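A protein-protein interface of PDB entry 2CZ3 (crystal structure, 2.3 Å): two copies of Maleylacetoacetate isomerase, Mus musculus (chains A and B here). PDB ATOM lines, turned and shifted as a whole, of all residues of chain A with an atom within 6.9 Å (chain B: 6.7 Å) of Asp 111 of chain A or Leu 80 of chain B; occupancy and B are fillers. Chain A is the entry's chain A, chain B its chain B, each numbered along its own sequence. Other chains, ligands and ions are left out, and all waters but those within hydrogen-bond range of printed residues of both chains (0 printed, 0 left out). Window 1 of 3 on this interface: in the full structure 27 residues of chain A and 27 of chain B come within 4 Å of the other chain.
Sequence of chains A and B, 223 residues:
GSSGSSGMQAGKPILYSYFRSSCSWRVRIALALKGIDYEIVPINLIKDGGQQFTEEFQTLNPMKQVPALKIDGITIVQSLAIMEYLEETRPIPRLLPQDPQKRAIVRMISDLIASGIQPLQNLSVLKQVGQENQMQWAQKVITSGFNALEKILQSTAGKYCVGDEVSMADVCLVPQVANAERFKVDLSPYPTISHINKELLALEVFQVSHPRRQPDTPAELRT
The backbone NH of Val 77 of chain B lies close to the side-chain sulfur of Met 108 of chain A (3.8 Å). The side-chain hydroxyl (OG) of Ser 115 of chain A lies within hydrogen-bond range of the side-chain hydroxyl (OG) of Ser 115 of chain B (2.7 Å).
The side-chain carboxylate of Glu 84 of chain A lies within salt-bridge range of the guanidinium group of Arg 107 of chain A (2.6 Å). The backbone NH (N) of Gly 116 of chain A is in hydrogen-bond range of the backbone carbonyl oxygen (O) of Asp 111 of chain A. The backbone NH (N) of Ile 117 of chain A sits at hydrogen-bond distance from the backbone carbonyl oxygen (O) of Leu 112 of chain A.
Among the printed residues, pairs that only touch across the chains: Leu 80 of chain A with Asp 111 of chain B, Leu 80 of chain A with Ser 115 of chain B, Ala 104 of chain A with Ala 81 of chain B, Arg 107 of chain A with Ala 81 of chain B, Arg 107 of chain A with Glu 84 of chain B, Met 108 of chain A with Gln 78 of chain B, Met 108 of chain A with Ala 81 of chain B, Asp 111 of chain A with Gln 78 of chain B, Asp 111 of chain A with Leu 80 of chain B, Asp 111 of chain A with Ala 81 of chain B, Leu 112 of chain A with Gln 78 of chain B, Ala 114 of chain A with Ser 115 of chain B, Ser 115 of chain A with Ala 114 of chain B and Pro 119 of chain A with Ser 115 of chain B.
Printed residues of chain B within 4 Å of Leu 80 of chain A: Asp 111 and Ser 115. Of chain B, only Gln 78 (3.4 Å), Leu 80 (3.7 Å) and Ala 81 (3.5 Å) come within 4 Å of Asp 111 of chain A. Printed residues of chain B within 4 Å of Leu 112 of chain A: Gln 78. Of the printed residues of chain B, Ser 115 of chain A touches Ala 114 and Ser 115. Of chain A, only Asp 111 comes within 4 Å of Leu 80 of chain B. The nearest residue of chain B that does not touch Asp 111 of chain A is Asp 111 of chain B (5.6 Å). The nearest residue of chain A that does not touch Leu 80 of chain B is Ser 115 of chain A (4.2 Å). The nearest printed residue of chain B that does not touch Ser 115 of chain A is Gln 78 of chain B (4.1 Å).
Of the 17 printed residues of chain B, 8 touch a printed residue of chain A. Hydrophobic or aromatic side chains of chain B that line the printed part of chain A: Val 77, Leu 80 and Ala 81. Printed residues of chain A that touch a printed residue of chain B: Leu 80, Ala 104, Arg 107, Met 108, Asp 111, Leu 112, Ala 114, Ser 115 and Pro 119. Hydrophobic or aromatic side chains of chain A that line the printed part of chain B: Leu 80, Met 108 and Pro 119. Among the printed residues, 16 pairs touch across the chains. Among the printed residues, no Asp or Glu carboxylate lies within 4 Å of a Lys or Arg side-chain nitrogen of the other chain.
Leu 80 of chain A touches Asp 111 of chain B, and with the chains exchanged Asp 111 of chain A touches Leu 80 of chain B. Leu 80 of chain A touches Ser 115 of chain B, but with the chains exchanged Ser 115 of chain A does not touch Leu 80 of chain B (4.2 Å). Ala 114 of chain A touches Ser 115 of chain B, and with the chains exchanged Ser 115 of chain A touches Ala 114 of chain B. Ser 115 of chain B touches its own counterpart, Ser 115 of chain A. 8 positions are printed for both chains. Of the 16 pairs that touch across the chains among the printed residues, 5 have their exchanged pair printed and touching as well.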
ATOM      1  N   LEU A  80      -6.581  20.650   0.720  1.00  0.00           N
ATOM      2  CA  LEU A  80      -6.738  20.369  -0.710  1.00  0.00           C
ATOM      3  C   LEU A  80      -7.027  18.872  -0.909  1.00  0.00           C
ATOM      4  O   LEU A  80      -7.969  18.499  -1.603  1.00  0.00           O
ATOM      5  CB  LEU A  80      -5.495  20.784  -1.477  1.00  0.00           C
ATOM      6  CG  LEU A  80      -5.262  22.291  -1.508  1.00  0.00           C
ATOM      7  CD1 LEU A  80      -3.818  22.530  -1.865  1.00  0.00           C
ATOM      8  CD2 LEU A  80      -6.173  23.025  -2.469  1.00  0.00           C
ATOM      9  N   GLU A  84     -10.511  17.109  -2.300  1.00  0.00           N
ATOM     10  CA  GLU A  84     -10.490  16.223  -3.455  1.00  0.00           C
ATOM     11  C   GLU A  84     -11.055  14.834  -3.111  1.00  0.00           C
ATOM     12  O   GLU A  84     -11.648  14.165  -3.957  1.00  0.00           O
ATOM     13  CB  GLU A  84      -9.068  16.119  -4.023  1.00  0.00           C
ATOM     14  CG  GLU A  84      -8.532  17.451  -4.587  1.00  0.00           C
ATOM     15  CD  GLU A  84      -8.690  17.586  -6.088  1.00  0.00           C
ATOM     16  OE1 GLU A  84      -9.433  16.793  -6.684  1.00  0.00           O
ATOM     17  OE2 GLU A  84      -8.057  18.486  -6.686  1.00  0.00           O
ATOM     18  N   ALA A 104      -8.924  22.732 -14.396  1.00  0.00           N
ATOM     19  CA  ALA A 104      -7.583  23.255 -14.214  1.00  0.00           C
ATOM     20  C   ALA A 104      -7.618  24.713 -13.749  1.00  0.00           C
ATOM     21  O   ALA A 104      -6.796  25.090 -12.923  1.00  0.00           O
ATOM     22  CB  ALA A 104      -6.799  23.129 -15.492  1.00  0.00           C
ATOM     23  N   VAL A 106     -10.047  26.127 -11.974  1.00  0.00           N
ATOM     24  CA  VAL A 106     -10.585  26.119 -10.618  1.00  0.00           C
ATOM     25  C   VAL A 106      -9.472  25.711  -9.655  1.00  0.00           C
ATOM     26  O   VAL A 106      -9.320  26.303  -8.590  1.00  0.00           O
ATOM     27  CB  VAL A 106     -11.847  25.201 -10.536  1.00  0.00           C
ATOM     28  CG1 VAL A 106     -12.156  24.748  -9.102  1.00  0.00           C
ATOM     29  CG2 VAL A 106     -13.029  25.918 -11.134  1.00  0.00           C
ATOM     30  N   ARG A 107      -8.685  24.723 -10.079  1.00  0.00           N
ATOM     31  CA  ARG A 107      -7.516  24.243  -9.332  1.00  0.00           C
ATOM     32  C   ARG A 107      -6.387  25.264  -9.259  1.00  0.00           C
ATOM     33  O   ARG A 107      -5.762  25.414  -8.227  1.00  0.00           O
ATOM     34  CB  ARG A 107      -7.012  22.926  -9.946  1.00  0.00           C
ATOM     35  CG  ARG A 107      -7.953  21.722  -9.682  1.00  0.00           C
ATOM     36  CD  ARG A 107      -7.260  20.399  -9.492  1.00  0.00           C
ATOM     37  NE  ARG A 107      -8.180  19.296  -9.193  1.00  0.00           N
ATOM     38  CZ  ARG A 107      -8.577  18.346 -10.070  1.00  0.00           C
ATOM     39  NH1 ARG A 107      -8.226  18.383 -11.344  1.00  0.00           N
ATOM     40  NH2 ARG A 107      -9.388  17.364  -9.671  1.00  0.00           N
ATOM     41  N   MET A 108      -6.138  25.978 -10.344  1.00  0.00           N
ATOM     42  CA  MET A 108      -5.150  27.074 -10.347  1.00  0.00           C
ATOM     43  C   MET A 108      -5.412  28.061  -9.243  1.00  0.00           C
ATOM     44  O   MET A 108      -4.511  28.371  -8.463  1.00  0.00           O
ATOM     45  CB  MET A 108      -5.236  27.861 -11.630  1.00  0.00           C
ATOM     46  CG  MET A 108      -4.396  27.346 -12.708  1.00  0.00           C
ATOM     47  SD  MET A 108      -4.961  28.175 -14.350  1.00  0.00           S
ATOM     48  CE  MET A 108      -4.456  29.986 -14.070  1.00  0.00           C
ATOM     49  N   ILE A 109      -6.652  28.554  -9.209  1.00  0.00           N
ATOM     50  CA  ILE A 109      -7.038  29.625  -8.290  1.00  0.00           C
ATOM     51  C   ILE A 109      -6.929  29.123  -6.879  1.00  0.00           C
ATOM     52  O   ILE A 109      -6.306  29.772  -6.048  1.00  0.00           O
ATOM     53  CB  ILE A 109      -8.448  30.160  -8.619  1.00  0.00           C
ATOM     54  CG1 ILE A 109      -8.400  30.885  -9.980  1.00  0.00           C
ATOM     55  CG2 ILE A 109      -8.941  31.107  -7.534  1.00  0.00           C
ATOM     56  CD1 ILE A 109      -9.700  30.830 -10.752  1.00  0.00           C
ATOM     57  N   SER A 110      -7.474  27.932  -6.652  1.00  0.00           N
ATOM     58  CA  SER A 110      -7.454  27.270  -5.351  1.00  0.00           C
ATOM     59  C   SER A 110      -6.046  27.107  -4.781  1.00  0.00           C
ATOM     60  O   SER A 110      -5.793  27.404  -3.608  1.00  0.00           O
ATOM     61  CB  SER A 110      -8.096  25.887  -5.491  1.00  0.00           C
ATOM     62  OG  SER A 110      -9.499  26.001  -5.638  1.00  0.00           O
ATOM     63  N   ASP A 111      -5.148  26.631  -5.634  1.00  0.00           N
ATOM     64  CA  ASP A 111      -3.771  26.382  -5.280  1.00  0.00           C
ATOM     65  C   ASP A 111      -2.987  27.678  -5.126  1.00  0.00           C
ATOM     66  O   ASP A 111      -2.105  27.769  -4.294  1.00  0.00           O
ATOM     67  CB  ASP A 111      -3.159  25.451  -6.326  1.00  0.00           C
ATOM     68  CG  ASP A 111      -3.834  24.058  -6.347  1.00  0.00           C
ATOM     69  OD1 ASP A 111      -4.292  23.600  -5.264  1.00  0.00           O
ATOM     70  OD2 ASP A 111      -3.931  23.333  -7.380  1.00  0.00           O
ATOM     71  N   LEU A 112      -3.331  28.685  -5.909  1.00  0.00           N
ATOM     72  CA  LEU A 112      -2.802  30.043  -5.741  1.00  0.00           C
ATOM     73  C   LEU A 112      -3.075  30.548  -4.326  1.00  0.00           C
ATOM     74  O   LEU A 112      -2.228  31.146  -3.688  1.00  0.00           O
ATOM     75  CB  LEU A 112      -3.484  30.963  -6.743  1.00  0.00           C
ATOM     76  CG  LEU A 112      -2.703  32.152  -7.274  1.00  0.00           C
ATOM     77  CD1 LEU A 112      -3.378  32.670  -8.563  1.00  0.00           C
ATOM     78  CD2 LEU A 112      -2.618  33.228  -6.226  1.00  0.00           C
ATOM     79  N   ILE A 113      -4.284  30.314  -3.851  1.00  0.00           N
ATOM     80  CA  ILE A 113      -4.636  30.677  -2.502  1.00  0.00           C
ATOM     81  C   ILE A 113      -3.910  29.763  -1.511  1.00  0.00           C
ATOM     82  O   ILE A 113      -3.138  30.242  -0.681  1.00  0.00           O
ATOM     83  CB  ILE A 113      -6.164  30.613  -2.311  1.00  0.00           C
ATOM     84  CG1 ILE A 113      -6.828  31.669  -3.200  1.00  0.00           C
ATOM     85  CG2 ILE A 113      -6.497  30.819  -0.855  1.00  0.00           C
ATOM     86  CD1 ILE A 113      -8.357  31.606  -3.263  1.00  0.00           C
ATOM     87  N   ALA A 114      -4.131  28.456  -1.628  1.00  0.00           N
ATOM     88  CA  ALA A 114      -3.645  27.484  -0.633  1.00  0.00           C
ATOM     89  C   ALA A 114      -2.138  27.286  -0.596  1.00  0.00           C
ATOM     90  O   ALA A 114      -1.589  26.939   0.450  1.00  0.00           O
ATOM     91  CB  ALA A 114      -4.292  26.118  -0.840  1.00  0.00           C
ATOM     92  N   SER A 115      -1.473  27.444  -1.733  1.00  0.00           N
ATOM     93  CA  SER A 115      -0.025  27.220  -1.807  1.00  0.00           C
ATOM     94  C   SER A 115       0.764  28.514  -1.916  1.00  0.00           C
ATOM     95  O   SER A 115       1.953  28.529  -1.630  1.00  0.00           O
ATOM     96  CB  SER A 115       0.340  26.322  -3.004  1.00  0.00           C
ATOM     97  OG  SER A 115      -0.209  25.008  -2.882  1.00  0.00           O
ATOM     98  N   GLY A 116       0.103  29.596  -2.330  1.00  0.00           N
ATOM     99  CA  GLY A 116       0.776  30.844  -2.672  1.00  0.00           C
ATOM    100  C   GLY A 116       0.558  31.965  -1.680  1.00  0.00           C
ATOM    101  O   GLY A 116       1.520  32.600  -1.229  1.00  0.00           O
ATOM    102  N   ILE A 117      -0.687  32.223  -1.311  1.00  0.00           N
ATOM    103  CA  ILE A 117      -0.959  33.327  -0.393  1.00  0.00           C
ATOM    104  C   ILE A 117      -0.915  32.883   1.065  1.00  0.00           C
ATOM    105  O   ILE A 117      -0.192  33.452   1.874  1.00  0.00           O
ATOM    106  CB  ILE A 117      -2.284  33.985  -0.706  1.00  0.00           C
ATOM    107  CG1 ILE A 117      -2.295  34.464  -2.159  1.00  0.00           C
ATOM    108  CG2 ILE A 117      -2.532  35.152   0.277  1.00  0.00           C
ATOM    109  CD1 ILE A 117      -3.677  34.847  -2.681  1.00  0.00           C
ATOM    110  N   PRO A 119       0.120  30.134   2.960  1.00  0.00           N
ATOM    111  CA  PRO A 119       1.332  29.661   3.653  1.00  0.00           C
ATOM    112  C   PRO A 119       2.299  30.771   3.985  1.00  0.00           C
ATOM    113  O   PRO A 119       3.005  30.666   4.982  1.00  0.00           O
ATOM    114  CB  PRO A 119       1.987  28.710   2.642  1.00  0.00           C
ATOM    115  CG  PRO A 119       0.925  28.355   1.707  1.00  0.00           C
ATOM    116  CD  PRO A 119       0.013  29.546   1.612  1.00  0.00           C
ATOM    117  N   MET A 168     -14.403  24.776  -5.870  1.00  0.00           N
ATOM    118  CA  MET A 168     -13.289  24.756  -4.911  1.00  0.00           C
ATOM    119  C   MET A 168     -12.590  26.121  -4.771  1.00  0.00           C
ATOM    120  O   MET A 168     -12.083  26.441  -3.692  1.00  0.00           O
ATOM    121  CB  MET A 168     -12.278  23.712  -5.349  1.00  0.00           C
ATOM    122  CG  MET A 168     -11.064  23.593  -4.482  1.00  0.00           C
ATOM    123  SD  MET A 168     -10.260  21.848  -4.652  1.00  0.00           S
ATOM    124  CE  MET A 168      -8.520  22.299  -5.265  1.00  0.00           C
ATOM    125  N   CYS A 172     -11.945  28.313  -1.232  1.00  0.00           N
ATOM    126  CA  CYS A 172     -10.629  28.853  -0.877  1.00  0.00           C
ATOM    127  C   CYS A 172     -10.649  30.384  -0.746  1.00  0.00           C
ATOM    128  O   CYS A 172      -9.892  30.966   0.028  1.00  0.00           O
ATOM    129  CB  CYS A 172      -9.605  28.471  -1.967  1.00  0.00           C
ATOM    130  SG  CYS A 172      -9.157  26.702  -2.102  1.00  0.00           S
ATOM    131  N   ARG B  26       8.842  19.393 -11.060  1.00  0.00           N
ATOM    132  CA  ARG B  26       7.689  18.532 -10.899  1.00  0.00           C
ATOM    133  C   ARG B  26       6.960  18.330 -12.219  1.00  0.00           C
ATOM    134  O   ARG B  26       6.590  17.223 -12.585  1.00  0.00           O
ATOM    135  CB  ARG B  26       6.696  19.138  -9.923  1.00  0.00           C
ATOM    136  CG  ARG B  26       7.085  19.080  -8.446  1.00  0.00           C
ATOM    137  CD  ARG B  26       6.077  19.802  -7.570  1.00  0.00           C
ATOM    138  NE  ARG B  26       6.686  20.539  -6.464  1.00  0.00           N
ATOM    139  CZ  ARG B  26       6.123  21.564  -5.827  1.00  0.00           C
ATOM    140  NH1 ARG B  26       4.915  22.018  -6.162  1.00  0.00           N
ATOM    141  NH2 ARG B  26       6.781  22.148  -4.836  1.00  0.00           N
ATOM    142  N   VAL B  27       6.715  19.425 -12.914  1.00  0.00           N
ATOM    143  CA  VAL B  27       5.949  19.374 -14.141  1.00  0.00           C
ATOM    144  C   VAL B  27       6.798  18.705 -15.241  1.00  0.00           C
ATOM    145  O   VAL B  27       6.262  17.999 -16.075  1.00  0.00           O
ATOM    146  CB  VAL B  27       5.425  20.778 -14.524  1.00  0.00           C
ATOM    147  CG1 VAL B  27       4.840  20.814 -15.914  1.00  0.00           C
ATOM    148  CG2 VAL B  27       4.361  21.218 -13.521  1.00  0.00           C
ATOM    149  N   VAL B  77      -1.274  27.481 -14.722  1.00  0.00           N
ATOM    150  CA  VAL B  77      -0.222  27.701 -13.725  1.00  0.00           C
ATOM    151  C   VAL B  77      -0.526  26.856 -12.496  1.00  0.00           C
ATOM    152  O   VAL B  77      -1.631  26.324 -12.353  1.00  0.00           O
ATOM    153  CB  VAL B  77      -0.086  29.189 -13.308  1.00  0.00           C
ATOM    154  CG1 VAL B  77       0.243  30.033 -14.522  1.00  0.00           C
ATOM    155  CG2 VAL B  77      -1.354  29.706 -12.600  1.00  0.00           C
ATOM    156  N   GLN B  78       0.456  26.753 -11.611  1.00  0.00           N
ATOM    157  CA  GLN B  78       0.352  25.945 -10.408  1.00  0.00           C
ATOM    158  C   GLN B  78       0.583  24.479 -10.750  1.00  0.00           C
ATOM    159  O   GLN B  78      -0.291  23.820 -11.309  1.00  0.00           O
ATOM    160  CB  GLN B  78      -1.026  26.110  -9.723  1.00  0.00           C
ATOM    161  CG  GLN B  78      -1.226  27.441  -9.045  1.00  0.00           C
ATOM    162  CD  GLN B  78      -0.249  27.635  -7.898  1.00  0.00           C
ATOM    163  OE1 GLN B  78      -0.052  26.723  -7.087  1.00  0.00           O
ATOM    164  NE2 GLN B  78       0.375  28.812  -7.834  1.00  0.00           N
ATOM    165  N   SER B  79       1.756  23.975 -10.384  1.00  0.00           N
ATOM    166  CA  SER B  79       2.157  22.588 -10.629  1.00  0.00           C
ATOM    167  C   SER B  79       1.129  21.527 -10.239  1.00  0.00           C
ATOM    168  O   SER B  79       1.003  20.515 -10.928  1.00  0.00           O
ATOM    169  CB  SER B  79       3.469  22.296  -9.883  1.00  0.00           C
ATOM    170  OG  SER B  79       3.257  22.231  -8.478  1.00  0.00           O
ATOM    171  N   LEU B  80       0.426  21.718  -9.131  1.00  0.00           N
ATOM    172  CA  LEU B  80      -0.548  20.719  -8.707  1.00  0.00           C
ATOM    173  C   LEU B  80      -1.703  20.641  -9.740  1.00  0.00           C
ATOM    174  O   LEU B  80      -2.041  19.555 -10.220  1.00  0.00           O
ATOM    175  CB  LEU B  80      -1.057  21.006  -7.300  1.00  0.00           C
ATOM    176  CG  LEU B  80      -0.464  20.299  -6.065  1.00  0.00           C
ATOM    177  CD1 LEU B  80       0.869  19.595  -6.279  1.00  0.00           C
ATOM    178  CD2 LEU B  80      -0.380  21.326  -4.898  1.00  0.00           C
ATOM    179  N   ALA B  81      -2.255  21.795 -10.091  1.00  0.00           N
ATOM    180  CA  ALA B  81      -3.264  21.931 -11.146  1.00  0.00           C
ATOM    181  C   ALA B  81      -2.815  21.337 -12.475  1.00  0.00           C
ATOM    182  O   ALA B  81      -3.566  20.621 -13.121  1.00  0.00           O
ATOM    183  CB  ALA B  81      -3.584  23.411 -11.357  1.00  0.00           C
ATOM    184  N   ILE B  82      -1.585  21.652 -12.881  1.00  0.00           N
ATOM    185  CA  ILE B  82      -1.022  21.141 -14.129  1.00  0.00           C
ATOM    186  C   ILE B  82      -0.938  19.607 -14.111  1.00  0.00           C
ATOM    187  O   ILE B  82      -1.299  18.954 -15.074  1.00  0.00           O
ATOM    188  CB  ILE B  82       0.364  21.760 -14.376  1.00  0.00           C
ATOM    189  CG1 ILE B  82       0.230  23.251 -14.736  1.00  0.00           C
ATOM    190  CG2 ILE B  82       1.114  21.008 -15.474  1.00  0.00           C
ATOM    191  CD1 ILE B  82       1.336  24.101 -14.166  1.00  0.00           C
ATOM    192  N   MET B  83      -0.467  19.029 -13.017  1.00  0.00           N
ATOM    193  CA  MET B  83      -0.341  17.574 -12.934  1.00  0.00           C
ATOM    194  C   MET B  83      -1.729  16.897 -12.889  1.00  0.00           C
ATOM    195  O   MET B  83      -1.899  15.847 -13.471  1.00  0.00           O
ATOM    196  CB  MET B  83       0.528  17.146 -11.734  1.00  0.00           C
ATOM    197  CG  MET B  83       1.995  17.655 -11.774  1.00  0.00           C
ATOM    198  SD  MET B  83       3.191  16.896 -10.365  1.00  0.00           S
ATOM    199  CE  MET B  83       2.712  17.980  -8.888  1.00  0.00           C
ATOM    200  N   GLU B  84      -2.716  17.477 -12.210  1.00  0.00           N
ATOM    201  CA  GLU B  84      -4.059  16.886 -12.216  1.00  0.00           C
ATOM    202  C   GLU B  84      -4.620  16.889 -13.646  1.00  0.00           C
ATOM    203  O   GLU B  84      -5.269  15.954 -14.089  1.00  0.00           O
ATOM    204  CB  GLU B  84      -5.040  17.631 -11.291  1.00  0.00           C
ATOM    205  CG  GLU B  84      -4.673  17.775  -9.786  1.00  0.00           C
ATOM    206  CD  GLU B  84      -4.981  16.569  -8.894  1.00  0.00           C
ATOM    207  OE1 GLU B  84      -5.698  15.624  -9.285  1.00  0.00           O
ATOM    208  OE2 GLU B  84      -4.472  16.569  -7.758  1.00  0.00           O
ATOM    209  N   TYR B  85      -4.369  17.959 -14.373  1.00  0.00           N
ATOM    210  CA  TYR B  85      -4.871  18.071 -15.720  1.00  0.00           C
ATOM    211  C   TYR B  85      -4.214  16.989 -16.583  1.00  0.00           C
ATOM    212  O   TYR B  85      -4.881  16.320 -17.364  1.00  0.00           O
ATOM    213  CB  TYR B  85      -4.585  19.462 -16.268  1.00  0.00           C
ATOM    214  CG  TYR B  85      -5.023  19.631 -17.688  1.00  0.00           C
ATOM    215  CD1 TYR B  85      -6.359  19.852 -18.005  1.00  0.00           C
ATOM    216  CD2 TYR B  85      -4.100  19.534 -18.729  1.00  0.00           C
ATOM    217  CE1 TYR B  85      -6.772  19.985 -19.338  1.00  0.00           C
ATOM    218  CE2 TYR B  85      -4.483  19.679 -20.060  1.00  0.00           C
ATOM    219  CZ  TYR B  85      -5.816  19.909 -20.365  1.00  0.00           C
ATOM    220  OH  TYR B  85      -6.176  20.032 -21.702  1.00  0.00           O
ATOM    221  N   SER B 110       1.892  15.018  -1.330  1.00  0.00           N
ATOM    222  CA  SER B 110       2.135  16.022  -2.355  1.00  0.00           C
ATOM    223  C   SER B 110       1.838  17.413  -1.847  1.00  0.00           C
ATOM    224  O   SER B 110       2.623  18.312  -2.030  1.00  0.00           O
ATOM    225  CB  SER B 110       1.268  15.758  -3.605  1.00  0.00           C
ATOM    226  OG  SER B 110       1.489  14.459  -4.141  1.00  0.00           O
ATOM    227  N   ASP B 111       0.687  17.584  -1.211  1.00  0.00           N
ATOM    228  CA  ASP B 111       0.234  18.890  -0.727  1.00  0.00           C
ATOM    229  C   ASP B 111       1.063  19.345   0.461  1.00  0.00           C
ATOM    230  O   ASP B 111       1.335  20.530   0.637  1.00  0.00           O
ATOM    231  CB  ASP B 111      -1.251  18.844  -0.317  1.00  0.00           C
ATOM    232  CG  ASP B 111      -2.181  18.760  -1.514  1.00  0.00           C
ATOM    233  OD1 ASP B 111      -1.838  19.328  -2.569  1.00  0.00           O
ATOM    234  OD2 ASP B 111      -3.262  18.145  -1.521  1.00  0.00           O
ATOM    235  N   ALA B 114       4.085  20.597  -1.482  1.00  0.00           N
ATOM    236  CA  ALA B 114       3.789  21.728  -2.350  1.00  0.00           C
ATOM    237  C   ALA B 114       3.166  22.911  -1.640  1.00  0.00           C
ATOM    238  O   ALA B 114       3.418  24.037  -2.043  1.00  0.00           O
ATOM    239  CB  ALA B 114       2.912  21.290  -3.490  1.00  0.00           C
ATOM    240  N   SER B 115       2.377  22.672  -0.596  1.00  0.00           N
ATOM    241  CA  SER B 115       1.686  23.766   0.134  1.00  0.00           C
ATOM    242  C   SER B 115       2.334  24.077   1.472  1.00  0.00           C
ATOM    243  O   SER B 115       2.184  25.178   1.982  1.00  0.00           O
ATOM    244  CB  SER B 115       0.215  23.429   0.367  1.00  0.00           C
ATOM    245  OG  SER B 115      -0.445  23.245  -0.868  1.00  0.00           O
ATOM    246  N   MET B 168       2.211  10.916  -7.699  1.00  0.00           N
ATOM    247  CA  MET B 168       2.391  12.371  -7.579  1.00  0.00           C
ATOM    248  C   MET B 168       3.290  12.728  -6.391  1.00  0.00           C
ATOM    249  O   MET B 168       3.997  13.725  -6.431  1.00  0.00           O
ATOM    250  CB  MET B 168       1.035  13.092  -7.459  1.00  0.00           C
ATOM    251  CG  MET B 168       1.083  14.592  -7.696  1.00  0.00           C
ATOM    252  SD  MET B 168      -0.658  15.505  -7.381  1.00  0.00           S
ATOM    253  CE  MET B 168      -1.359  15.378  -9.171  1.00  0.00           C
ATOM    254  N   CYS B 172       6.763  15.105  -6.352  1.00  0.00           N
ATOM    255  CA  CYS B 172       6.984  16.227  -5.436  1.00  0.00           C
ATOM    256  C   CYS B 172       8.180  16.018  -4.502  1.00  0.00           C
ATOM    257  O   CYS B 172       8.786  16.979  -4.004  1.00  0.00           O
ATOM    258  CB  CYS B 172       5.738  16.415  -4.590  1.00  0.00           C
ATOM    259  SG  CYS B 172       4.364  17.045  -5.562  1.00  0.00           S
